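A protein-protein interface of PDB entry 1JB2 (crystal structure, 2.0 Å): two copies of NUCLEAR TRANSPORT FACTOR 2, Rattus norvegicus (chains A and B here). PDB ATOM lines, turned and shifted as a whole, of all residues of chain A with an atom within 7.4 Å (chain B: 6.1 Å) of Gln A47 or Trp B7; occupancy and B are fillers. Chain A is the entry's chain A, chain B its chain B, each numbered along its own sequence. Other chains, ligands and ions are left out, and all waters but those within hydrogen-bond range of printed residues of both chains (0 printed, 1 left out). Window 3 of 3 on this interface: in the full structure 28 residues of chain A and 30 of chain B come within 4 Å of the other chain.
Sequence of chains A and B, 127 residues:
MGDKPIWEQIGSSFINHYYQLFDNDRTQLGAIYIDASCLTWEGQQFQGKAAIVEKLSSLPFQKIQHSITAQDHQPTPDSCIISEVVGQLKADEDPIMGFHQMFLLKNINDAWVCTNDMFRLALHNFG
Gln A47 touches just one residue of chain B: Trp B7 (3.4 Å).
Trp B7 touches just one residue of chain A: Gln A47 (3.4 Å).
Printed residues of chain A within 4 Å of Gln B74: Cys A38, Leu A39 and Thr A40.
Of the printed residues of chain B, Cys A38 touches Gln B74 (3.4 Å).
Printed residues of chain B within 4 Å of Leu A39: Gln B74.
Of the printed residues of chain B, Thr A40 touches Gln B74 (2.7 Å).
Glu B8 touches none of the printed residues of chain A.
Ser B83 touches none of the printed residues of chain A.
The nearest printed residue of chain B that does not touch Leu A39 is His B73 (7.5 Å).
Of the 15 printed residues of chain A, 4 touch a printed residue of chain B.
Hydrophobic or aromatic side chains of chain B that line the printed part of chain A: Trp B7.
Among the printed residues, pairs that only touch across the chains: Leu A39 with Gln B74 (3.3 Å) and Gln A47 with Trp B7 (3.4 Å).
No position is printed for both chains.
Of the 4 pairs that touch across the chains among the printed residues, none has its exchanged pair printed and touching as well.
The backbone NH (N) of Phe A46 is in hydrogen-bond range of the backbone carbonyl oxygen (O) of Leu A39 (2.8 Å).
The side-chain hydroxyl (OG1) of Thr A40 sits at hydrogen-bond distance from the side-chain amide nitrogen (NE2) of Gln B74 (2.7 Å).
The backbone carbonyl oxygen (O) of Cys A38 sits close to the side-chain amide oxygen (OE1) of Gln B74 (3.4 Å).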
ATOM      1  N   ASP A  35       3.449 -11.947   3.873  1.00  0.00           N
ATOM      2  CA  ASP A  35       2.017 -12.194   3.633  1.00  0.00           C
ATOM      3  C   ASP A  35       1.561 -13.635   3.815  1.00  0.00           C
ATOM      4  O   ASP A  35       0.457 -13.886   4.305  1.00  0.00           O
ATOM      5  CB  ASP A  35       1.591 -11.680   2.247  1.00  0.00           C
ATOM      6  CG  ASP A  35       1.529 -10.165   2.195  1.00  0.00           C
ATOM      7  OD1 ASP A  35       1.258  -9.548   3.252  1.00  0.00           O
ATOM      8  OD2 ASP A  35       1.739  -9.586   1.116  1.00  0.00           O
ATOM      9  N   ALA A  36       2.417 -14.581   3.456  1.00  0.00           N
ATOM     10  CA  ALA A  36       2.055 -15.984   3.597  1.00  0.00           C
ATOM     11  C   ALA A  36       2.347 -16.561   4.981  1.00  0.00           C
ATOM     12  O   ALA A  36       2.053 -17.719   5.229  1.00  0.00           O
ATOM     13  CB  ALA A  36       2.764 -16.824   2.532  1.00  0.00           C
ATOM     14  N   SER A  37       2.927 -15.773   5.880  1.00  0.00           N
ATOM     15  CA  SER A  37       3.226 -16.294   7.206  1.00  0.00           C
ATOM     16  C   SER A  37       1.941 -16.741   7.884  1.00  0.00           C
ATOM     17  O   SER A  37       0.869 -16.157   7.655  1.00  0.00           O
ATOM     18  CB  SER A  37       3.895 -15.227   8.085  1.00  0.00           C
ATOM     19  OG  SER A  37       5.171 -14.882   7.609  1.00  0.00           O
ATOM     20  N   CYS A  38       2.052 -17.790   8.696  1.00  0.00           N
ATOM     21  CA  CYS A  38       0.916 -18.313   9.436  1.00  0.00           C
ATOM     22  C   CYS A  38       1.286 -18.397  10.891  1.00  0.00           C
ATOM     23  O   CYS A  38       2.437 -18.701  11.238  1.00  0.00           O
ATOM     24  CB  CYS A  38       0.516 -19.713   8.957  1.00  0.00           C
ATOM     25  SG  CYS A  38      -0.344 -19.730   7.391  1.00  0.00           S
ATOM     26  N   LEU A  39       0.301 -18.140  11.748  1.00  0.00           N
ATOM     27  CA  LEU A  39       0.498 -18.211  13.181  1.00  0.00           C
ATOM     28  C   LEU A  39      -0.593 -19.041  13.844  1.00  0.00           C
ATOM     29  O   LEU A  39      -1.744 -19.037  13.403  1.00  0.00           O
ATOM     30  CB  LEU A  39       0.478 -16.809  13.805  1.00  0.00           C
ATOM     31  CG  LEU A  39       0.244 -16.737  15.332  1.00  0.00           C
ATOM     32  CD1 LEU A  39       1.542 -17.137  16.080  1.00  0.00           C
ATOM     33  CD2 LEU A  39      -0.189 -15.319  15.746  1.00  0.00           C
ATOM     34  N   THR A  40      -0.211 -19.795  14.873  1.00  0.00           N
ATOM     35  CA  THR A  40      -1.194 -20.526  15.666  1.00  0.00           C
ATOM     36  C   THR A  40      -0.870 -20.067  17.068  1.00  0.00           C
ATOM     37  O   THR A  40       0.245 -20.272  17.551  1.00  0.00           O
ATOM     38  CB  THR A  40      -1.072 -22.040  15.583  1.00  0.00           C
ATOM     39  OG1 THR A  40      -1.159 -22.458  14.215  1.00  0.00           O
ATOM     40  CG2 THR A  40      -2.233 -22.671  16.349  1.00  0.00           C
ATOM     41  N   GLN A  44      -5.328 -21.373  18.387  1.00  0.00           N
ATOM     42  CA  GLN A  44      -6.179 -20.629  17.453  1.00  0.00           C
ATOM     43  C   GLN A  44      -5.349 -20.211  16.229  1.00  0.00           C
ATOM     44  O   GLN A  44      -4.231 -19.727  16.370  1.00  0.00           O
ATOM     45  CB  GLN A  44      -6.750 -19.383  18.134  1.00  0.00           C
ATOM     46  CG  GLN A  44      -7.717 -18.575  17.251  1.00  0.00           C
ATOM     47  CD  GLN A  44      -9.089 -19.227  17.122  1.00  0.00           C
ATOM     48  OE1 GLN A  44      -9.821 -19.365  18.113  1.00  0.00           O
ATOM     49  NE2 GLN A  44      -9.446 -19.630  15.901  1.00  0.00           N
ATOM     50  N   GLN A  45      -5.912 -20.359  15.036  1.00  0.00           N
ATOM     51  CA  GLN A  45      -5.177 -20.029  13.820  1.00  0.00           C
ATOM     52  C   GLN A  45      -5.364 -18.638  13.234  1.00  0.00           C
ATOM     53  O   GLN A  45      -6.474 -18.108  13.171  1.00  0.00           O
ATOM     54  CB  GLN A  45      -5.519 -21.033  12.730  1.00  0.00           C
ATOM     55  CG  GLN A  45      -5.694 -22.435  13.215  1.00  0.00           C
ATOM     56  CD  GLN A  45      -6.543 -23.231  12.261  1.00  0.00           C
ATOM     57  OE1 GLN A  45      -6.109 -23.552  11.152  1.00  0.00           O
ATOM     58  NE2 GLN A  45      -7.773 -23.532  12.668  1.00  0.00           N
ATOM     59  N   PHE A  46      -4.250 -18.062  12.801  1.00  0.00           N
ATOM     60  CA  PHE A  46      -4.231 -16.762  12.154  1.00  0.00           C
ATOM     61  C   PHE A  46      -3.327 -16.919  10.948  1.00  0.00           C
ATOM     62  O   PHE A  46      -2.103 -16.884  11.064  1.00  0.00           O
ATOM     63  CB  PHE A  46      -3.719 -15.674  13.111  1.00  0.00           C
ATOM     64  CG  PHE A  46      -4.544 -15.564  14.370  1.00  0.00           C
ATOM     65  CD1 PHE A  46      -4.247 -16.356  15.486  1.00  0.00           C
ATOM     66  CD2 PHE A  46      -5.689 -14.767  14.395  1.00  0.00           C
ATOM     67  CE1 PHE A  46      -5.087 -16.362  16.604  1.00  0.00           C
ATOM     68  CE2 PHE A  46      -6.537 -14.764  15.510  1.00  0.00           C
ATOM     69  CZ  PHE A  46      -6.237 -15.564  16.611  1.00  0.00           C
ATOM     70  N   GLN A  47      -3.956 -17.128   9.790  1.00  0.00           N
ATOM     71  CA  GLN A  47      -3.249 -17.301   8.526  1.00  0.00           C
ATOM     72  C   GLN A  47      -3.146 -15.955   7.812  1.00  0.00           C
ATOM     73  O   GLN A  47      -4.143 -15.221   7.676  1.00  0.00           O
ATOM     74  CB  GLN A  47      -3.998 -18.319   7.659  1.00  0.00           C
ATOM     75  CG  GLN A  47      -4.115 -19.683   8.323  1.00  0.00           C
ATOM     76  CD  GLN A  47      -5.236 -20.548   7.757  1.00  0.00           C
ATOM     77  OE1 GLN A  47      -5.944 -21.214   8.505  1.00  0.00           O
ATOM     78  NE2 GLN A  47      -5.387 -20.555   6.431  1.00  0.00           N
ATOM     79  N   GLY A  48      -1.932 -15.619   7.378  1.00  0.00           N
ATOM     80  CA  GLY A  48      -1.714 -14.360   6.694  1.00  0.00           C
ATOM     81  C   GLY A  48      -1.171 -13.318   7.659  1.00  0.00           C
ATOM     82  O   GLY A  48      -1.557 -13.276   8.829  1.00  0.00           O
ATOM     83  N   LYS A  49      -0.283 -12.473   7.154  1.00  0.00           N
ATOM     84  CA  LYS A  49       0.345 -11.434   7.944  1.00  0.00           C
ATOM     85  C   LYS A  49      -0.637 -10.499   8.631  1.00  0.00           C
ATOM     86  O   LYS A  49      -0.456 -10.164   9.810  1.00  0.00           O
ATOM     87  CB  LYS A  49       1.280 -10.596   7.055  1.00  0.00           C
ATOM     88  CG  LYS A  49       2.140  -9.600   7.825  1.00  0.00           C
ATOM     89  CD  LYS A  49       3.227  -8.964   6.944  1.00  0.00           C
ATOM     90  CE  LYS A  49       4.112  -8.020   7.761  1.00  0.00           C
ATOM     91  NZ  LYS A  49       5.314  -7.514   6.983  1.00  0.00           N
ATOM     92  N   ALA A  50      -1.657 -10.056   7.891  1.00  0.00           N
ATOM     93  CA  ALA A  50      -2.646  -9.127   8.439  1.00  0.00           C
ATOM     94  C   ALA A  50      -3.319  -9.633   9.700  1.00  0.00           C
ATOM     95  O   ALA A  50      -3.493  -8.876  10.664  1.00  0.00           O
ATOM     96  CB  ALA A  50      -3.721  -8.780   7.366  1.00  0.00           C
ATOM     97  N   ALA A  51      -3.736 -10.897   9.690  1.00  0.00           N
ATOM     98  CA  ALA A  51      -4.395 -11.472  10.858  1.00  0.00           C
ATOM     99  C   ALA A  51      -3.397 -11.651  11.998  1.00  0.00           C
ATOM    100  O   ALA A  51      -3.742 -11.482  13.167  1.00  0.00           O
ATOM    101  CB  ALA A  51      -5.038 -12.828  10.501  1.00  0.00           C
ATOM    102  N   ILE A  52      -2.165 -12.022  11.659  1.00  0.00           N
ATOM    103  CA  ILE A  52      -1.130 -12.218  12.679  1.00  0.00           C
ATOM    104  C   ILE A  52      -0.895 -10.882  13.371  1.00  0.00           C
ATOM    105  O   ILE A  52      -0.926 -10.792  14.601  1.00  0.00           O
ATOM    106  CB  ILE A  52       0.207 -12.709  12.042  1.00  0.00           C
ATOM    107  CG1 ILE A  52       0.005 -14.086  11.399  1.00  0.00           C
ATOM    108  CG2 ILE A  52       1.321 -12.747  13.108  1.00  0.00           C
ATOM    109  CD1 ILE A  52       1.284 -14.698  10.843  1.00  0.00           C
ATOM    110  N   PRO B   5      -8.762 -27.707   6.578  1.00  0.00           N
ATOM    111  CA  PRO B   5      -8.060 -27.472   5.311  1.00  0.00           C
ATOM    112  C   PRO B   5      -7.232 -28.706   4.954  1.00  0.00           C
ATOM    113  O   PRO B   5      -6.951 -29.537   5.813  1.00  0.00           O
ATOM    114  CB  PRO B   5      -7.160 -26.279   5.620  1.00  0.00           C
ATOM    115  CG  PRO B   5      -7.874 -25.576   6.732  1.00  0.00           C
ATOM    116  CD  PRO B   5      -8.367 -26.712   7.589  1.00  0.00           C
ATOM    117  N   ILE B   6      -6.815 -28.800   3.699  1.00  0.00           N
ATOM    118  CA  ILE B   6      -6.041 -29.934   3.236  1.00  0.00           C
ATOM    119  C   ILE B   6      -4.724 -30.189   4.005  1.00  0.00           C
ATOM    120  O   ILE B   6      -4.347 -31.342   4.212  1.00  0.00           O
ATOM    121  CB  ILE B   6      -5.759 -29.803   1.710  1.00  0.00           C
ATOM    122  CG1 ILE B   6      -5.125 -31.094   1.198  1.00  0.00           C
ATOM    123  CG2 ILE B   6      -4.880 -28.594   1.423  1.00  0.00           C
ATOM    124  CD1 ILE B   6      -6.028 -32.310   1.385  1.00  0.00           C
ATOM    125  N   TRP B   7      -4.029 -29.137   4.432  1.00  0.00           N
ATOM    126  CA  TRP B   7      -2.782 -29.350   5.164  1.00  0.00           C
ATOM    127  C   TRP B   7      -3.071 -30.009   6.518  1.00  0.00           C
ATOM    128  O   TRP B   7      -2.266 -30.798   7.005  1.00  0.00           O
ATOM    129  CB  TRP B   7      -2.001 -28.026   5.332  1.00  0.00           C
ATOM    130  CG  TRP B   7      -2.795 -26.892   5.931  1.00  0.00           C
ATOM    131  CD1 TRP B   7      -3.030 -26.672   7.251  1.00  0.00           C
ATOM    132  CD2 TRP B   7      -3.449 -25.831   5.224  1.00  0.00           C
ATOM    133  NE1 TRP B   7      -3.786 -25.539   7.420  1.00  0.00           N
ATOM    134  CE2 TRP B   7      -4.057 -25.000   6.190  1.00  0.00           C
ATOM    135  CE3 TRP B   7      -3.583 -25.500   3.863  1.00  0.00           C
ATOM    136  CZ2 TRP B   7      -4.787 -23.853   5.843  1.00  0.00           C
ATOM    137  CZ3 TRP B   7      -4.306 -24.366   3.521  1.00  0.00           C
ATOM    138  CH2 TRP B   7      -4.900 -23.553   4.510  1.00  0.00           C
ATOM    139  N   GLU B   8      -4.228 -29.713   7.113  1.00  0.00           N
ATOM    140  CA  GLU B   8      -4.590 -30.328   8.401  1.00  0.00           C
ATOM    141  C   GLU B   8      -4.989 -31.801   8.225  1.00  0.00           C
ATOM    142  O   GLU B   8      -4.708 -32.633   9.079  1.00  0.00           O
ATOM    143  CB  GLU B   8      -5.743 -29.567   9.063  1.00  0.00           C
ATOM    144  CG  GLU B   8      -5.970 -29.936  10.531  1.00  0.00           C
ATOM    145  CD  GLU B   8      -7.305 -29.439  11.057  1.00  0.00           C
ATOM    146  OE1 GLU B   8      -7.673 -28.289  10.724  1.00  0.00           O
ATOM    147  OE2 GLU B   8      -7.982 -30.199  11.800  1.00  0.00           O
ATOM    148  N   GLN B   9      -5.659 -32.114   7.120  1.00  0.00           N
ATOM    149  CA  GLN B   9      -6.059 -33.494   6.835  1.00  0.00           C
ATOM    150  C   GLN B   9      -4.811 -34.351   6.594  1.00  0.00           C
ATOM    151  O   GLN B   9      -4.704 -35.461   7.091  1.00  0.00           O
ATOM    152  CB  GLN B   9      -6.943 -33.546   5.577  1.00  0.00           C
ATOM    153  CG  GLN B   9      -8.245 -32.760   5.687  1.00  0.00           C
ATOM    154  CD  GLN B   9      -8.985 -32.687   4.370  1.00  0.00           C
ATOM    155  OE1 GLN B   9      -9.100 -33.681   3.660  1.00  0.00           O
ATOM    156  NE2 GLN B   9      -9.500 -31.505   4.040  1.00  0.00           N
ATOM    157  N   ILE B  10      -3.871 -33.821   5.814  1.00  0.00           N
ATOM    158  CA  ILE B  10      -2.648 -34.556   5.505  1.00  0.00           C
ATOM    159  C   ILE B  10      -1.798 -34.740   6.766  1.00  0.00           C
ATOM    160  O   ILE B  10      -1.322 -35.848   7.056  1.00  0.00           O
ATOM    161  CB  ILE B  10      -1.791 -33.787   4.450  1.00  0.00           C
ATOM    162  CG1 ILE B  10      -2.571 -33.631   3.146  1.00  0.00           C
ATOM    163  CG2 ILE B  10      -0.474 -34.496   4.207  1.00  0.00           C
ATOM    164  CD1 ILE B  10      -3.032 -34.902   2.585  1.00  0.00           C
ATOM    165  N   GLY B  11      -1.606 -33.643   7.500  1.00  0.00           N
ATOM    166  CA  GLY B  11      -0.779 -33.661   8.702  1.00  0.00           C
ATOM    167  C   GLY B  11      -1.334 -34.567   9.779  1.00  0.00           C
ATOM    168  O   GLY B  11      -0.607 -35.349  10.398  1.00  0.00           O
ATOM    169  N   SER B  12      -2.634 -34.449  10.020  1.00  0.00           N
ATOM    170  CA  SER B  12      -3.305 -35.284  11.023  1.00  0.00           C
ATOM    171  C   SER B  12      -3.173 -36.761  10.642  1.00  0.00           C
ATOM    172  O   SER B  12      -2.991 -37.639  11.495  1.00  0.00           O
ATOM    173  CB  SER B  12      -4.788 -34.918  11.092  1.00  0.00           C
ATOM    174  OG  SER B  12      -5.391 -35.631  12.146  1.00  0.00           O
ATOM    175  N   HIS B  73      -1.476 -27.833  12.736  1.00  0.00           N
ATOM    176  CA  HIS B  73      -0.845 -27.981  11.413  1.00  0.00           C
ATOM    177  C   HIS B  73      -0.947 -26.710  10.588  1.00  0.00           C
ATOM    178  O   HIS B  73      -1.975 -26.035  10.602  1.00  0.00           O
ATOM    179  CB  HIS B  73      -1.529 -29.114  10.645  1.00  0.00           C
ATOM    180  CG  HIS B  73      -1.605 -30.398  11.409  1.00  0.00           C
ATOM    181  ND1 HIS B  73      -0.629 -31.370  11.330  1.00  0.00           N
ATOM    182  CD2 HIS B  73      -2.526 -30.859  12.290  1.00  0.00           C
ATOM    183  CE1 HIS B  73      -0.945 -32.372  12.129  1.00  0.00           C
ATOM    184  NE2 HIS B  73      -2.091 -32.091  12.721  1.00  0.00           N
ATOM    185  N   GLN B  74       0.108 -26.393   9.848  1.00  0.00           N
ATOM    186  CA  GLN B  74       0.111 -25.204   9.011  1.00  0.00           C
ATOM    187  C   GLN B  74       0.769 -25.481   7.653  1.00  0.00           C
ATOM    188  O   GLN B  74       1.593 -26.398   7.516  1.00  0.00           O
ATOM    189  CB  GLN B  74       0.919 -24.062   9.656  1.00  0.00           C
ATOM    190  CG  GLN B  74       0.360 -23.420  10.918  1.00  0.00           C
ATOM    191  CD  GLN B  74       1.298 -22.369  11.494  1.00  0.00           C
ATOM    192  OE1 GLN B  74       2.389 -22.129  10.965  1.00  0.00           O
ATOM    193  NE2 GLN B  74       0.883 -21.744  12.590  1.00  0.00           N
ATOM    194  N   PRO B  75       0.397 -24.697   6.627  1.00  0.00           N
ATOM    195  CA  PRO B  75       1.012 -24.891   5.312  1.00  0.00           C
ATOM    196  C   PRO B  75       2.225 -23.939   5.292  1.00  0.00           C
ATOM    197  O   PRO B  75       2.224 -22.916   6.003  1.00  0.00           O
ATOM    198  CB  PRO B  75      -0.093 -24.469   4.349  1.00  0.00           C
ATOM    199  CG  PRO B  75      -0.770 -23.346   5.088  1.00  0.00           C
ATOM    200  CD  PRO B  75      -0.771 -23.789   6.550  1.00  0.00           C
ATOM    201  N   CYS B  80       5.238 -27.276   2.124  1.00  0.00           N
ATOM    202  CA  CYS B  80       5.433 -28.286   3.132  1.00  0.00           C
ATOM    203  C   CYS B  80       4.337 -28.108   4.162  1.00  0.00           C
ATOM    204  O   CYS B  80       3.536 -27.178   4.079  1.00  0.00           O
ATOM    205  CB  CYS B  80       6.792 -28.140   3.812  1.00  0.00           C
ATOM    206  SG  CYS B  80       8.191 -28.501   2.709  1.00  0.00           S
ATOM    207  N   ILE B  81       4.304 -29.013   5.128  1.00  0.00           N
ATOM    208  CA  ILE B  81       3.334 -28.941   6.215  1.00  0.00           C
ATOM    209  C   ILE B  81       4.137 -29.035   7.502  1.00  0.00           C
ATOM    210  O   ILE B  81       4.994 -29.921   7.645  1.00  0.00           O
ATOM    211  CB  ILE B  81       2.317 -30.103   6.162  1.00  0.00           C
ATOM    212  CG1 ILE B  81       1.481 -30.001   4.878  1.00  0.00           C
ATOM    213  CG2 ILE B  81       1.393 -30.050   7.400  1.00  0.00           C
ATOM    214  CD1 ILE B  81       0.613 -31.212   4.610  1.00  0.00           C
ATOM    215  N   SER B  83       3.877 -29.481  11.544  1.00  0.00           N
ATOM    216  CA  SER B  83       2.970 -30.053  12.535  1.00  0.00           C
ATOM    217  C   SER B  83       3.550 -30.102  13.947  1.00  0.00           C
ATOM    218  O   SER B  83       4.725 -30.405  14.143  1.00  0.00           O
ATOM    219  CB  SER B  83       2.604 -31.485  12.116  1.00  0.00           C
ATOM    220  OG  SER B  83       2.053 -31.527  10.800  1.00  0.00           O
